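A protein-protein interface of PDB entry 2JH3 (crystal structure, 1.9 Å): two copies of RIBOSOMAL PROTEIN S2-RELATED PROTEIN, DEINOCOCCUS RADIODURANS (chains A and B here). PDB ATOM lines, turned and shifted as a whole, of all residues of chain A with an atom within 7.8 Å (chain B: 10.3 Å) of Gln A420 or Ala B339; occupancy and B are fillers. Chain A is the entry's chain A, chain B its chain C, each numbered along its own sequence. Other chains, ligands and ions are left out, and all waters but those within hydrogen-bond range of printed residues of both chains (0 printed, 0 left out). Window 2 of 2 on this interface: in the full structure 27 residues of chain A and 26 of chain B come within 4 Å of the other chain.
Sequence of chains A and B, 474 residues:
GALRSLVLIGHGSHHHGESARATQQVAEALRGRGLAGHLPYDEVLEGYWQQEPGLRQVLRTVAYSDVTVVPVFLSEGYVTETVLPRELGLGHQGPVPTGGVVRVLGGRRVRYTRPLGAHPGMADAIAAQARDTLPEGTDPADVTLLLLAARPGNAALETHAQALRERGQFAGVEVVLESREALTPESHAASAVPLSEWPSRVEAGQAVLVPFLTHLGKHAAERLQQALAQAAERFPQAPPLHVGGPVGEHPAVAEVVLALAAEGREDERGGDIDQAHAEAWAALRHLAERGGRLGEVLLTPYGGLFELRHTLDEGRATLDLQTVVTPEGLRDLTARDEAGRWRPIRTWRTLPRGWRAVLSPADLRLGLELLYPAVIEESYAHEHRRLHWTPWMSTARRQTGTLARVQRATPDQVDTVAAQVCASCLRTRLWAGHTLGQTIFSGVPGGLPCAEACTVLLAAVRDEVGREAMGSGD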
ATOM      1  N   TRP A 348      21.297  -4.307  27.395  1.00  0.00           N
ATOM      2  CA  TRP A 348      22.537  -4.979  27.082  1.00  0.00           C
ATOM      3  C   TRP A 348      23.465  -4.891  28.269  1.00  0.00           C
ATOM      4  O   TRP A 348      23.450  -3.901  29.010  1.00  0.00           O
ATOM      5  CB  TRP A 348      23.173  -4.461  25.766  1.00  0.00           C
ATOM      6  CG  TRP A 348      22.586  -5.150  24.614  1.00  0.00           C
ATOM      7  CD1 TRP A 348      21.295  -5.619  24.515  1.00  0.00           C
ATOM      8  CD2 TRP A 348      23.194  -5.406  23.365  1.00  0.00           C
ATOM      9  NE1 TRP A 348      21.108  -6.206  23.309  1.00  0.00           N
ATOM     10  CE2 TRP A 348      22.270  -6.121  22.595  1.00  0.00           C
ATOM     11  CE3 TRP A 348      24.496  -5.229  22.870  1.00  0.00           C
ATOM     12  CZ2 TRP A 348      22.556  -6.551  21.284  1.00  0.00           C
ATOM     13  CZ3 TRP A 348      24.799  -5.682  21.611  1.00  0.00           C
ATOM     14  CH2 TRP A 348      23.846  -6.354  20.829  1.00  0.00           C
ATOM     15  N   VAL A 414      16.530 -17.505  12.310  1.00  0.00           N
ATOM     16  CA  VAL A 414      16.283 -16.546  13.403  1.00  0.00           C
ATOM     17  C   VAL A 414      16.784 -17.051  14.747  1.00  0.00           C
ATOM     18  O   VAL A 414      17.315 -16.262  15.478  1.00  0.00           O
ATOM     19  CB  VAL A 414      14.980 -15.751  13.397  1.00  0.00           C
ATOM     20  CG1 VAL A 414      14.150 -15.911  12.154  1.00  0.00           C
ATOM     21  CG2 VAL A 414      14.202 -15.775  14.723  1.00  0.00           C
ATOM     22  N   ASP A 415      16.637 -18.355  15.045  1.00  0.00           N
ATOM     23  CA  ASP A 415      17.116 -18.931  16.283  1.00  0.00           C
ATOM     24  C   ASP A 415      18.623 -18.835  16.414  1.00  0.00           C
ATOM     25  O   ASP A 415      19.201 -18.591  17.496  1.00  0.00           O
ATOM     26  CB  ASP A 415      16.661 -20.375  16.388  1.00  0.00           C
ATOM     27  CG  ASP A 415      15.205 -20.525  16.723  1.00  0.00           C
ATOM     28  OD1 ASP A 415      14.442 -19.562  17.011  1.00  0.00           O
ATOM     29  OD2 ASP A 415      14.786 -21.684  16.720  1.00  0.00           O
ATOM     30  N   THR A 416      19.318 -18.989  15.307  1.00  0.00           N
ATOM     31  CA  THR A 416      20.742 -18.895  15.293  1.00  0.00           C
ATOM     32  C   THR A 416      21.285 -17.487  15.516  1.00  0.00           C
ATOM     33  O   THR A 416      22.284 -17.272  16.263  1.00  0.00           O
ATOM     34  CB  THR A 416      21.202 -19.448  13.912  1.00  0.00           C
ATOM     35  OG1 THR A 416      20.904 -20.867  13.891  1.00  0.00           O
ATOM     36  CG2 THR A 416      22.574 -19.246  13.717  1.00  0.00           C
ATOM     37  N   VAL A 417      20.642 -16.502  14.869  1.00  0.00           N
ATOM     38  CA  VAL A 417      21.017 -15.108  15.056  1.00  0.00           C
ATOM     39  C   VAL A 417      20.626 -14.618  16.452  1.00  0.00           C
ATOM     40  O   VAL A 417      21.428 -13.986  17.081  1.00  0.00           O
ATOM     41  CB  VAL A 417      20.379 -14.204  13.966  1.00  0.00           C
ATOM     42  CG1 VAL A 417      20.746 -12.715  14.162  1.00  0.00           C
ATOM     43  CG2 VAL A 417      20.816 -14.684  12.588  1.00  0.00           C
ATOM     44  N   ALA A 418      19.431 -14.958  16.927  1.00  0.00           N
ATOM     45  CA  ALA A 418      19.013 -14.538  18.245  1.00  0.00           C
ATOM     46  C   ALA A 418      19.954 -15.083  19.314  1.00  0.00           C
ATOM     47  O   ALA A 418      20.311 -14.353  20.244  1.00  0.00           O
ATOM     48  CB  ALA A 418      17.631 -14.934  18.480  1.00  0.00           C
ATOM     49  N   ALA A 419      20.444 -16.319  19.189  1.00  0.00           N
ATOM     50  CA  ALA A 419      21.399 -16.859  20.198  1.00  0.00           C
ATOM     51  C   ALA A 419      22.657 -16.008  20.257  1.00  0.00           C
ATOM     52  O   ALA A 419      23.191 -15.706  21.328  1.00  0.00           O
ATOM     53  CB  ALA A 419      21.779 -18.326  19.890  1.00  0.00           C
ATOM     54  N   GLN A 420      23.085 -15.517  19.104  1.00  0.00           N
ATOM     55  CA  GLN A 420      24.303 -14.690  19.019  1.00  0.00           C
ATOM     56  C   GLN A 420      24.077 -13.260  19.484  1.00  0.00           C
ATOM     57  O   GLN A 420      24.897 -12.719  20.232  1.00  0.00           O
ATOM     58  CB  GLN A 420      24.864 -14.693  17.614  1.00  0.00           C
ATOM     59  CG  GLN A 420      25.461 -16.045  17.141  1.00  0.00           C
ATOM     60  CD  GLN A 420      26.491 -16.732  18.116  1.00  0.00           C
ATOM     61  OE1 GLN A 420      27.513 -16.146  18.481  1.00  0.00           O
ATOM     62  NE2 GLN A 420      26.161 -18.007  18.551  1.00  0.00           N
ATOM     63  N   VAL A 421      22.993 -12.634  19.042  1.00  0.00           N
ATOM     64  CA  VAL A 421      22.697 -11.234  19.411  1.00  0.00           C
ATOM     65  C   VAL A 421      22.205 -11.081  20.856  1.00  0.00           C
ATOM     66  O   VAL A 421      22.753 -10.319  21.637  1.00  0.00           O
ATOM     67  CB  VAL A 421      21.604 -10.726  18.523  1.00  0.00           C
ATOM     68  CG1 VAL A 421      21.037  -9.355  19.011  1.00  0.00           C
ATOM     69  CG2 VAL A 421      22.202 -10.534  17.134  1.00  0.00           C
ATOM     70  N   CYS A 422      21.237 -11.889  21.207  1.00  0.00           N
ATOM     71  CA  CYS A 422      20.590 -11.783  22.497  1.00  0.00           C
ATOM     72  C   CYS A 422      21.488 -12.168  23.689  1.00  0.00           C
ATOM     73  O   CYS A 422      21.195 -11.825  24.848  1.00  0.00           O
ATOM     74  CB  CYS A 422      19.328 -12.611  22.521  1.00  0.00           C
ATOM     75  SG  CYS A 422      18.077 -12.114  21.330  1.00  0.00           S
ATOM     76  N   ALA A 423      22.596 -12.871  23.395  1.00  0.00           N
ATOM     77  CA  ALA A 423      23.600 -13.162  24.424  1.00  0.00           C
ATOM     78  C   ALA A 423      24.166 -11.958  25.091  1.00  0.00           C
ATOM     79  O   ALA A 423      24.690 -12.038  26.226  1.00  0.00           O
ATOM     80  CB  ALA A 423      24.681 -14.010  23.845  1.00  0.00           C
ATOM     81  N   SER A 424      24.119 -10.821  24.403  1.00  0.00           N
ATOM     82  CA  SER A 424      24.548  -9.566  24.995  1.00  0.00           C
ATOM     83  C   SER A 424      23.541  -8.914  25.918  1.00  0.00           C
ATOM     84  O   SER A 424      23.872  -7.948  26.637  1.00  0.00           O
ATOM     85  CB  SER A 424      24.930  -8.592  23.873  1.00  0.00           C
ATOM     86  OG  SER A 424      26.176  -8.976  23.293  1.00  0.00           O
ATOM     87  N   CYS A 425      22.314  -9.415  25.890  1.00  0.00           N
ATOM     88  CA  CYS A 425      21.180  -8.782  26.508  1.00  0.00           C
ATOM     89  C   CYS A 425      20.854  -9.388  27.869  1.00  0.00           C
ATOM     90  O   CYS A 425      20.967 -10.608  28.044  1.00  0.00           O
ATOM     91  CB  CYS A 425      19.958  -8.969  25.592  1.00  0.00           C
ATOM     92  SG  CYS A 425      18.604  -7.812  25.935  1.00  0.00           S
ATOM     93  N   ARG A 429      13.937 -13.901  25.958  1.00  0.00           N
ATOM     94  CA  ARG A 429      13.026 -13.829  24.768  1.00  0.00           C
ATOM     95  C   ARG A 429      11.821 -14.705  24.881  1.00  0.00           C
ATOM     96  O   ARG A 429      11.760 -15.809  24.371  1.00  0.00           O
ATOM     97  CB  ARG A 429      13.822 -14.028  23.468  1.00  0.00           C
ATOM     98  CG  ARG A 429      14.639 -15.280  23.360  1.00  0.00           C
ATOM     99  CD  ARG A 429      15.566 -15.159  22.151  1.00  0.00           C
ATOM    100  NE  ARG A 429      16.410 -16.339  21.876  1.00  0.00           N
ATOM    101  CZ  ARG A 429      17.576 -16.565  22.471  1.00  0.00           C
ATOM    102  NH1 ARG A 429      18.297 -17.612  22.114  1.00  0.00           N
ATOM    103  NH2 ARG A 429      18.063 -15.734  23.406  1.00  0.00           N
ATOM    104  N   LEU A 457      18.143  -6.830  16.715  1.00  0.00           N
ATOM    105  CA  LEU A 457      18.017  -8.199  16.264  1.00  0.00           C
ATOM    106  C   LEU A 457      17.446  -8.277  14.842  1.00  0.00           C
ATOM    107  O   LEU A 457      17.927  -9.091  14.043  1.00  0.00           O
ATOM    108  CB  LEU A 457      17.105  -9.016  17.204  1.00  0.00           C
ATOM    109  CG  LEU A 457      16.759 -10.454  16.756  1.00  0.00           C
ATOM    110  CD1 LEU A 457      18.065 -11.258  16.563  1.00  0.00           C
ATOM    111  CD2 LEU A 457      15.919 -11.173  17.794  1.00  0.00           C
ATOM    112  N   ALA A 460      20.233  -7.563  12.448  1.00  0.00           N
ATOM    113  CA  ALA A 460      21.191  -8.710  12.417  1.00  0.00           C
ATOM    114  C   ALA A 460      20.613  -9.864  11.564  1.00  0.00           C
ATOM    115  O   ALA A 460      21.359 -10.550  10.811  1.00  0.00           O
ATOM    116  CB  ALA A 460      21.506  -9.182  13.841  1.00  0.00           C
ATOM    117  N   HIS B  15      39.076 -19.201  20.108  1.00  0.00           N
ATOM    118  CA  HIS B  15      37.804 -19.589  19.495  1.00  0.00           C
ATOM    119  C   HIS B  15      37.302 -21.027  19.691  1.00  0.00           C
ATOM    120  O   HIS B  15      36.100 -21.245  19.657  1.00  0.00           O
ATOM    121  CB  HIS B  15      37.870 -19.292  17.993  1.00  0.00           C
ATOM    122  CG  HIS B  15      37.953 -17.825  17.699  1.00  0.00           C
ATOM    123  ND1 HIS B  15      36.881 -16.969  17.879  1.00  0.00           N
ATOM    124  CD2 HIS B  15      38.970 -17.061  17.257  1.00  0.00           C
ATOM    125  CE1 HIS B  15      37.260 -15.731  17.613  1.00  0.00           C
ATOM    126  NE2 HIS B  15      38.510 -15.766  17.195  1.00  0.00           N
ATOM    127  N   LEU B 333      31.331 -25.293  32.903  1.00  0.00           N
ATOM    128  CA  LEU B 333      30.073 -24.467  32.771  1.00  0.00           C
ATOM    129  C   LEU B 333      30.315 -22.975  32.426  1.00  0.00           C
ATOM    130  O   LEU B 333      29.378 -22.288  31.942  1.00  0.00           O
ATOM    131  CB  LEU B 333      29.204 -24.616  34.031  1.00  0.00           C
ATOM    132  CG  LEU B 333      28.007 -25.617  34.167  1.00  0.00           C
ATOM    133  CD1 LEU B 333      28.183 -26.815  33.346  1.00  0.00           C
ATOM    134  CD2 LEU B 333      27.592 -25.962  35.591  1.00  0.00           C
ATOM    135  N   ALA B 335      33.090 -21.838  30.607  1.00  0.00           N
ATOM    136  CA  ALA B 335      34.027 -21.758  29.445  1.00  0.00           C
ATOM    137  C   ALA B 335      33.455 -21.074  28.234  1.00  0.00           C
ATOM    138  O   ALA B 335      34.191 -20.640  27.348  1.00  0.00           O
ATOM    139  CB  ALA B 335      34.490 -23.204  29.068  1.00  0.00           C
ATOM    140  N   ARG B 336      32.126 -21.038  28.106  1.00  0.00           N
ATOM    141  CA  ARG B 336      31.498 -20.376  26.998  1.00  0.00           C
ATOM    142  C   ARG B 336      30.446 -19.366  27.502  1.00  0.00           C
ATOM    143  O   ARG B 336      29.891 -19.551  28.533  1.00  0.00           O
ATOM    144  CB  ARG B 336      30.826 -21.385  26.106  1.00  0.00           C
ATOM    145  CG  ARG B 336      31.787 -22.384  25.449  1.00  0.00           C
ATOM    146  CD  ARG B 336      30.997 -23.539  24.790  1.00  0.00           C
ATOM    147  NE  ARG B 336      31.932 -24.542  24.285  1.00  0.00           N
ATOM    148  CZ  ARG B 336      32.744 -24.374  23.219  1.00  0.00           C
ATOM    149  NH1 ARG B 336      32.759 -23.247  22.479  1.00  0.00           N
ATOM    150  NH2 ARG B 336      33.586 -25.364  22.875  1.00  0.00           N
ATOM    151  N   ASP B 337      30.194 -18.332  26.721  1.00  0.00           N
ATOM    152  CA  ASP B 337      29.176 -17.330  27.030  1.00  0.00           C
ATOM    153  C   ASP B 337      27.796 -17.856  26.685  1.00  0.00           C
ATOM    154  O   ASP B 337      27.660 -19.008  26.265  1.00  0.00           O
ATOM    155  CB  ASP B 337      29.496 -16.003  26.304  1.00  0.00           C
ATOM    156  CG  ASP B 337      29.441 -16.072  24.756  1.00  0.00           C
ATOM    157  OD1 ASP B 337      28.813 -16.975  24.175  1.00  0.00           O
ATOM    158  OD2 ASP B 337      30.090 -15.153  24.104  1.00  0.00           O
ATOM    159  N   GLU B 338      26.770 -17.024  26.819  1.00  0.00           N
ATOM    160  CA  GLU B 338      25.398 -17.458  26.530  1.00  0.00           C
ATOM    161  C   GLU B 338      25.049 -17.805  25.083  1.00  0.00           C
ATOM    162  O   GLU B 338      24.076 -18.520  24.873  1.00  0.00           O
ATOM    163  CB  GLU B 338      24.369 -16.495  27.138  1.00  0.00           C
ATOM    164  CG  GLU B 338      24.355 -16.594  28.704  1.00  0.00           C
ATOM    165  CD  GLU B 338      23.577 -15.526  29.428  1.00  0.00           C
ATOM    166  OE1 GLU B 338      22.777 -14.869  28.763  1.00  0.00           O
ATOM    167  OE2 GLU B 338      23.834 -15.321  30.646  1.00  0.00           O
ATOM    168  N   ALA B 339      25.845 -17.347  24.129  1.00  0.00           N
ATOM    169  CA  ALA B 339      25.719 -17.717  22.704  1.00  0.00           C
ATOM    170  C   ALA B 339      26.494 -18.988  22.376  1.00  0.00           C
ATOM    171  O   ALA B 339      26.453 -19.406  21.231  1.00  0.00           O
ATOM    172  CB  ALA B 339      26.229 -16.630  21.839  1.00  0.00           C
ATOM    173  N   GLY B 340      27.234 -19.534  23.355  1.00  0.00           N
ATOM    174  CA  GLY B 340      28.055 -20.721  23.159  1.00  0.00           C
ATOM    175  C   GLY B 340      29.432 -20.479  22.638  1.00  0.00           C
ATOM    176  O   GLY B 340      30.106 -21.404  22.203  1.00  0.00           O
ATOM    177  N   ARG B 341      29.899 -19.252  22.737  1.00  0.00           N
ATOM    178  CA  ARG B 341      31.177 -18.879  22.140  1.00  0.00           C
ATOM    179  C   ARG B 341      32.225 -18.961  23.214  1.00  0.00           C
ATOM    180  O   ARG B 341      31.995 -18.638  24.365  1.00  0.00           O
ATOM    181  CB  ARG B 341      31.131 -17.468  21.652  1.00  0.00           C
ATOM    182  CG  ARG B 341      30.159 -17.193  20.605  1.00  0.00           C
ATOM    183  CD  ARG B 341      30.293 -15.692  20.215  1.00  0.00           C
ATOM    184  NE  ARG B 341      29.651 -14.786  21.204  1.00  0.00           N
ATOM    185  CZ  ARG B 341      28.670 -13.900  20.961  1.00  0.00           C
ATOM    186  NH1 ARG B 341      28.146 -13.693  19.743  1.00  0.00           N
ATOM    187  NH2 ARG B 341      28.198 -13.190  21.980  1.00  0.00           N
ATOM    188  N   TRP B 342      33.429 -19.387  22.829  1.00  0.00           N
ATOM    189  CA  TRP B 342      34.510 -19.618  23.804  1.00  0.00           C
ATOM    190  C   TRP B 342      34.858 -18.307  24.530  1.00  0.00           C
ATOM    191  O   TRP B 342      34.906 -17.212  23.897  1.00  0.00           O
ATOM    192  CB  TRP B 342      35.715 -20.182  23.005  1.00  0.00           C
ATOM    193  CG  TRP B 342      36.847 -20.753  23.763  1.00  0.00           C
ATOM    194  CD1 TRP B 342      38.099 -20.307  23.751  1.00  0.00           C
ATOM    195  CD2 TRP B 342      36.846 -21.928  24.552  1.00  0.00           C
ATOM    196  NE1 TRP B 342      38.893 -21.071  24.586  1.00  0.00           N
ATOM    197  CE2 TRP B 342      38.127 -22.083  25.073  1.00  0.00           C
ATOM    198  CE3 TRP B 342      35.844 -22.820  24.968  1.00  0.00           C
ATOM    199  CZ2 TRP B 342      38.456 -23.118  25.950  1.00  0.00           C
ATOM    200  CZ3 TRP B 342      36.188 -23.835  25.784  1.00  0.00           C
ATOM    201  CH2 TRP B 342      37.484 -23.963  26.297  1.00  0.00           C
ATOM    202  N   ARG B 343      35.317 -18.444  25.787  1.00  0.00           N
ATOM    203  CA  ARG B 343      35.785 -17.297  26.561  1.00  0.00           C
ATOM    204  C   ARG B 343      37.247 -17.412  26.896  1.00  0.00           C
ATOM    205  O   ARG B 343      37.581 -17.870  27.986  1.00  0.00           O
ATOM    206  CB  ARG B 343      34.981 -17.203  27.900  1.00  0.00           C
ATOM    207  CG  ARG B 343      33.459 -17.088  27.698  1.00  0.00           C
ATOM    208  CD  ARG B 343      32.610 -16.980  29.050  1.00  0.00           C
ATOM    209  NE  ARG B 343      32.940 -15.792  29.830  1.00  0.00           N
ATOM    210  CZ  ARG B 343      33.677 -15.769  30.893  1.00  0.00           C
ATOM    211  NH1 ARG B 343      34.048 -16.907  31.416  1.00  0.00           N
ATOM    212  NH2 ARG B 343      33.978 -14.609  31.502  1.00  0.00           N
ATOM    213  N   THR B 350      31.147 -11.533  30.327  1.00  0.00           N
ATOM    214  CA  THR B 350      30.391 -12.433  29.477  1.00  0.00           C
ATOM    215  C   THR B 350      30.078 -13.764  30.187  1.00  0.00           C
ATOM    216  O   THR B 350      29.709 -14.785  29.528  1.00  0.00           O
ATOM    217  CB  THR B 350      31.241 -12.697  28.176  1.00  0.00           C
ATOM    218  OG1 THR B 350      32.536 -13.151  28.537  1.00  0.00           O
ATOM    219  CG2 THR B 350      31.411 -11.435  27.357  1.00  0.00           C
ATOM    220  N   LEU B 351      30.340 -13.806  31.512  1.00  0.00           N
ATOM    221  CA  LEU B 351      30.080 -15.035  32.304  1.00  0.00           C
ATOM    222  C   LEU B 351      28.654 -15.417  32.050  1.00  0.00           C
ATOM    223  O   LEU B 351      27.833 -14.554  32.160  1.00  0.00           O
ATOM    224  CB  LEU B 351      30.358 -14.823  33.789  1.00  0.00           C
ATOM    225  CG  LEU B 351      30.537 -16.025  34.714  1.00  0.00           C
ATOM    226  CD1 LEU B 351      31.781 -16.856  34.370  1.00  0.00           C
ATOM    227  CD2 LEU B 351      30.657 -15.492  36.137  1.00  0.00           C
ATOM    228  N   PRO B 352      28.369 -16.684  31.697  1.00  0.00           N
ATOM    229  CA  PRO B 352      27.005 -17.100  31.456  1.00  0.00           C
ATOM    230  C   PRO B 352      26.191 -17.202  32.752  1.00  0.00           C
ATOM    231  O   PRO B 352      26.734 -17.474  33.837  1.00  0.00           O
ATOM    232  CB  PRO B 352      27.179 -18.469  30.801  1.00  0.00           C
ATOM    233  CG  PRO B 352      28.390 -19.028  31.409  1.00  0.00           C
ATOM    234  CD  PRO B 352      29.299 -17.802  31.470  1.00  0.00           C
ATOM    235  N   ARG B 353      24.897 -16.995  32.638  1.00  0.00           N
ATOM    236  CA  ARG B 353      23.980 -17.275  33.730  1.00  0.00           C
ATOM    237  C   ARG B 353      23.547 -18.769  33.724  1.00  0.00           C
ATOM    238  O   ARG B 353      23.886 -19.511  32.846  1.00  0.00           O
ATOM    239  CB  ARG B 353      22.764 -16.392  33.600  1.00  0.00           C
ATOM    240  CG  ARG B 353      23.047 -14.944  33.956  1.00  0.00           C
ATOM    241  CD  ARG B 353      21.826 -14.111  33.593  1.00  0.00           C
ATOM    242  NE  ARG B 353      21.753 -13.907  32.153  1.00  0.00           N
ATOM    243  CZ  ARG B 353      20.901 -13.106  31.528  1.00  0.00           C
ATOM    244  NH1 ARG B 353      20.019 -12.411  32.247  1.00  0.00           N
ATOM    245  NH2 ARG B 353      21.006 -12.961  30.195  1.00  0.00           N
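The backbone carbonyl oxygen (O) of Ala B339 is in hydrogen-bond range of the side-chain amide nitrogen (NE2) of Gln A420, 3.0 Å away.
The backbone carbonyl oxygen (O) of Cys A425 is in hydrogen-bond range of the guanidinium group (NH2) of Arg B353 (3.2 Å).
The guanidinium group (NH1) of Arg B341 is in hydrogen-bond range of the side-chain amide oxygen (OE1) of Gln A420 (2.8 Å).
The side-chain carboxylate (OD1) of Asp B337 sits at hydrogen-bond distance from the backbone NH (N) of Ala B339 (3.0 Å).
OE2 of Glu B338 lies within salt-bridge range of NE of Arg B353 (2.9 Å).
The side-chain carboxylate (OD2) of Asp B337 is in salt-bridge range of the guanidinium group (NE) of Arg B341 (3.0 Å).
No position is printed for both chains.
Of the 5 pairs that touch across the chains among the printed residues, none has its exchanged pair printed and touching as well.
Of the 15 printed residues of chain B, 3 touch a printed residue of chain A.
Hydrophobic or aromatic side chains of chain B within 4 Å of the printed part of chain A: Ala B339.
Among the printed residues, no Asp or Glu carboxylate lies within 4 Å of a Lys or Arg side-chain nitrogen of the other chain.
Ala A419 touches Ala B339 (O to CB, 3.2 Å).
Ala A423 touches Ala B339 (CB to N, 3.5 Å).
Gln A420 touches just these residues of chain B: Ala B339 and Arg B341.
Ala B339 touches three residues of chain A.
No residue of chain B comes within 4 Å of Ala A418.
Of chain B, only Ala B339 comes within 4 Å of Ala A419.
No residue of chain B comes within 4 Å of Val A421.
Of the printed residues of chain B, Cys A425 touches Arg B353 (3.2 Å).
Printed residues of chain A within 4 Å of Arg B353: Cys A425 (3.2 Å).
His B15 touches none of the printed residues of chain A.
Leu B351 touches none of the printed residues of chain A.
The nearest residue of chain B that does not touch Gln A420 is Gly B340 (5.2 Å).
The nearest residue of chain A that does not touch Ala B339 is Val A421 (5.9 Å).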
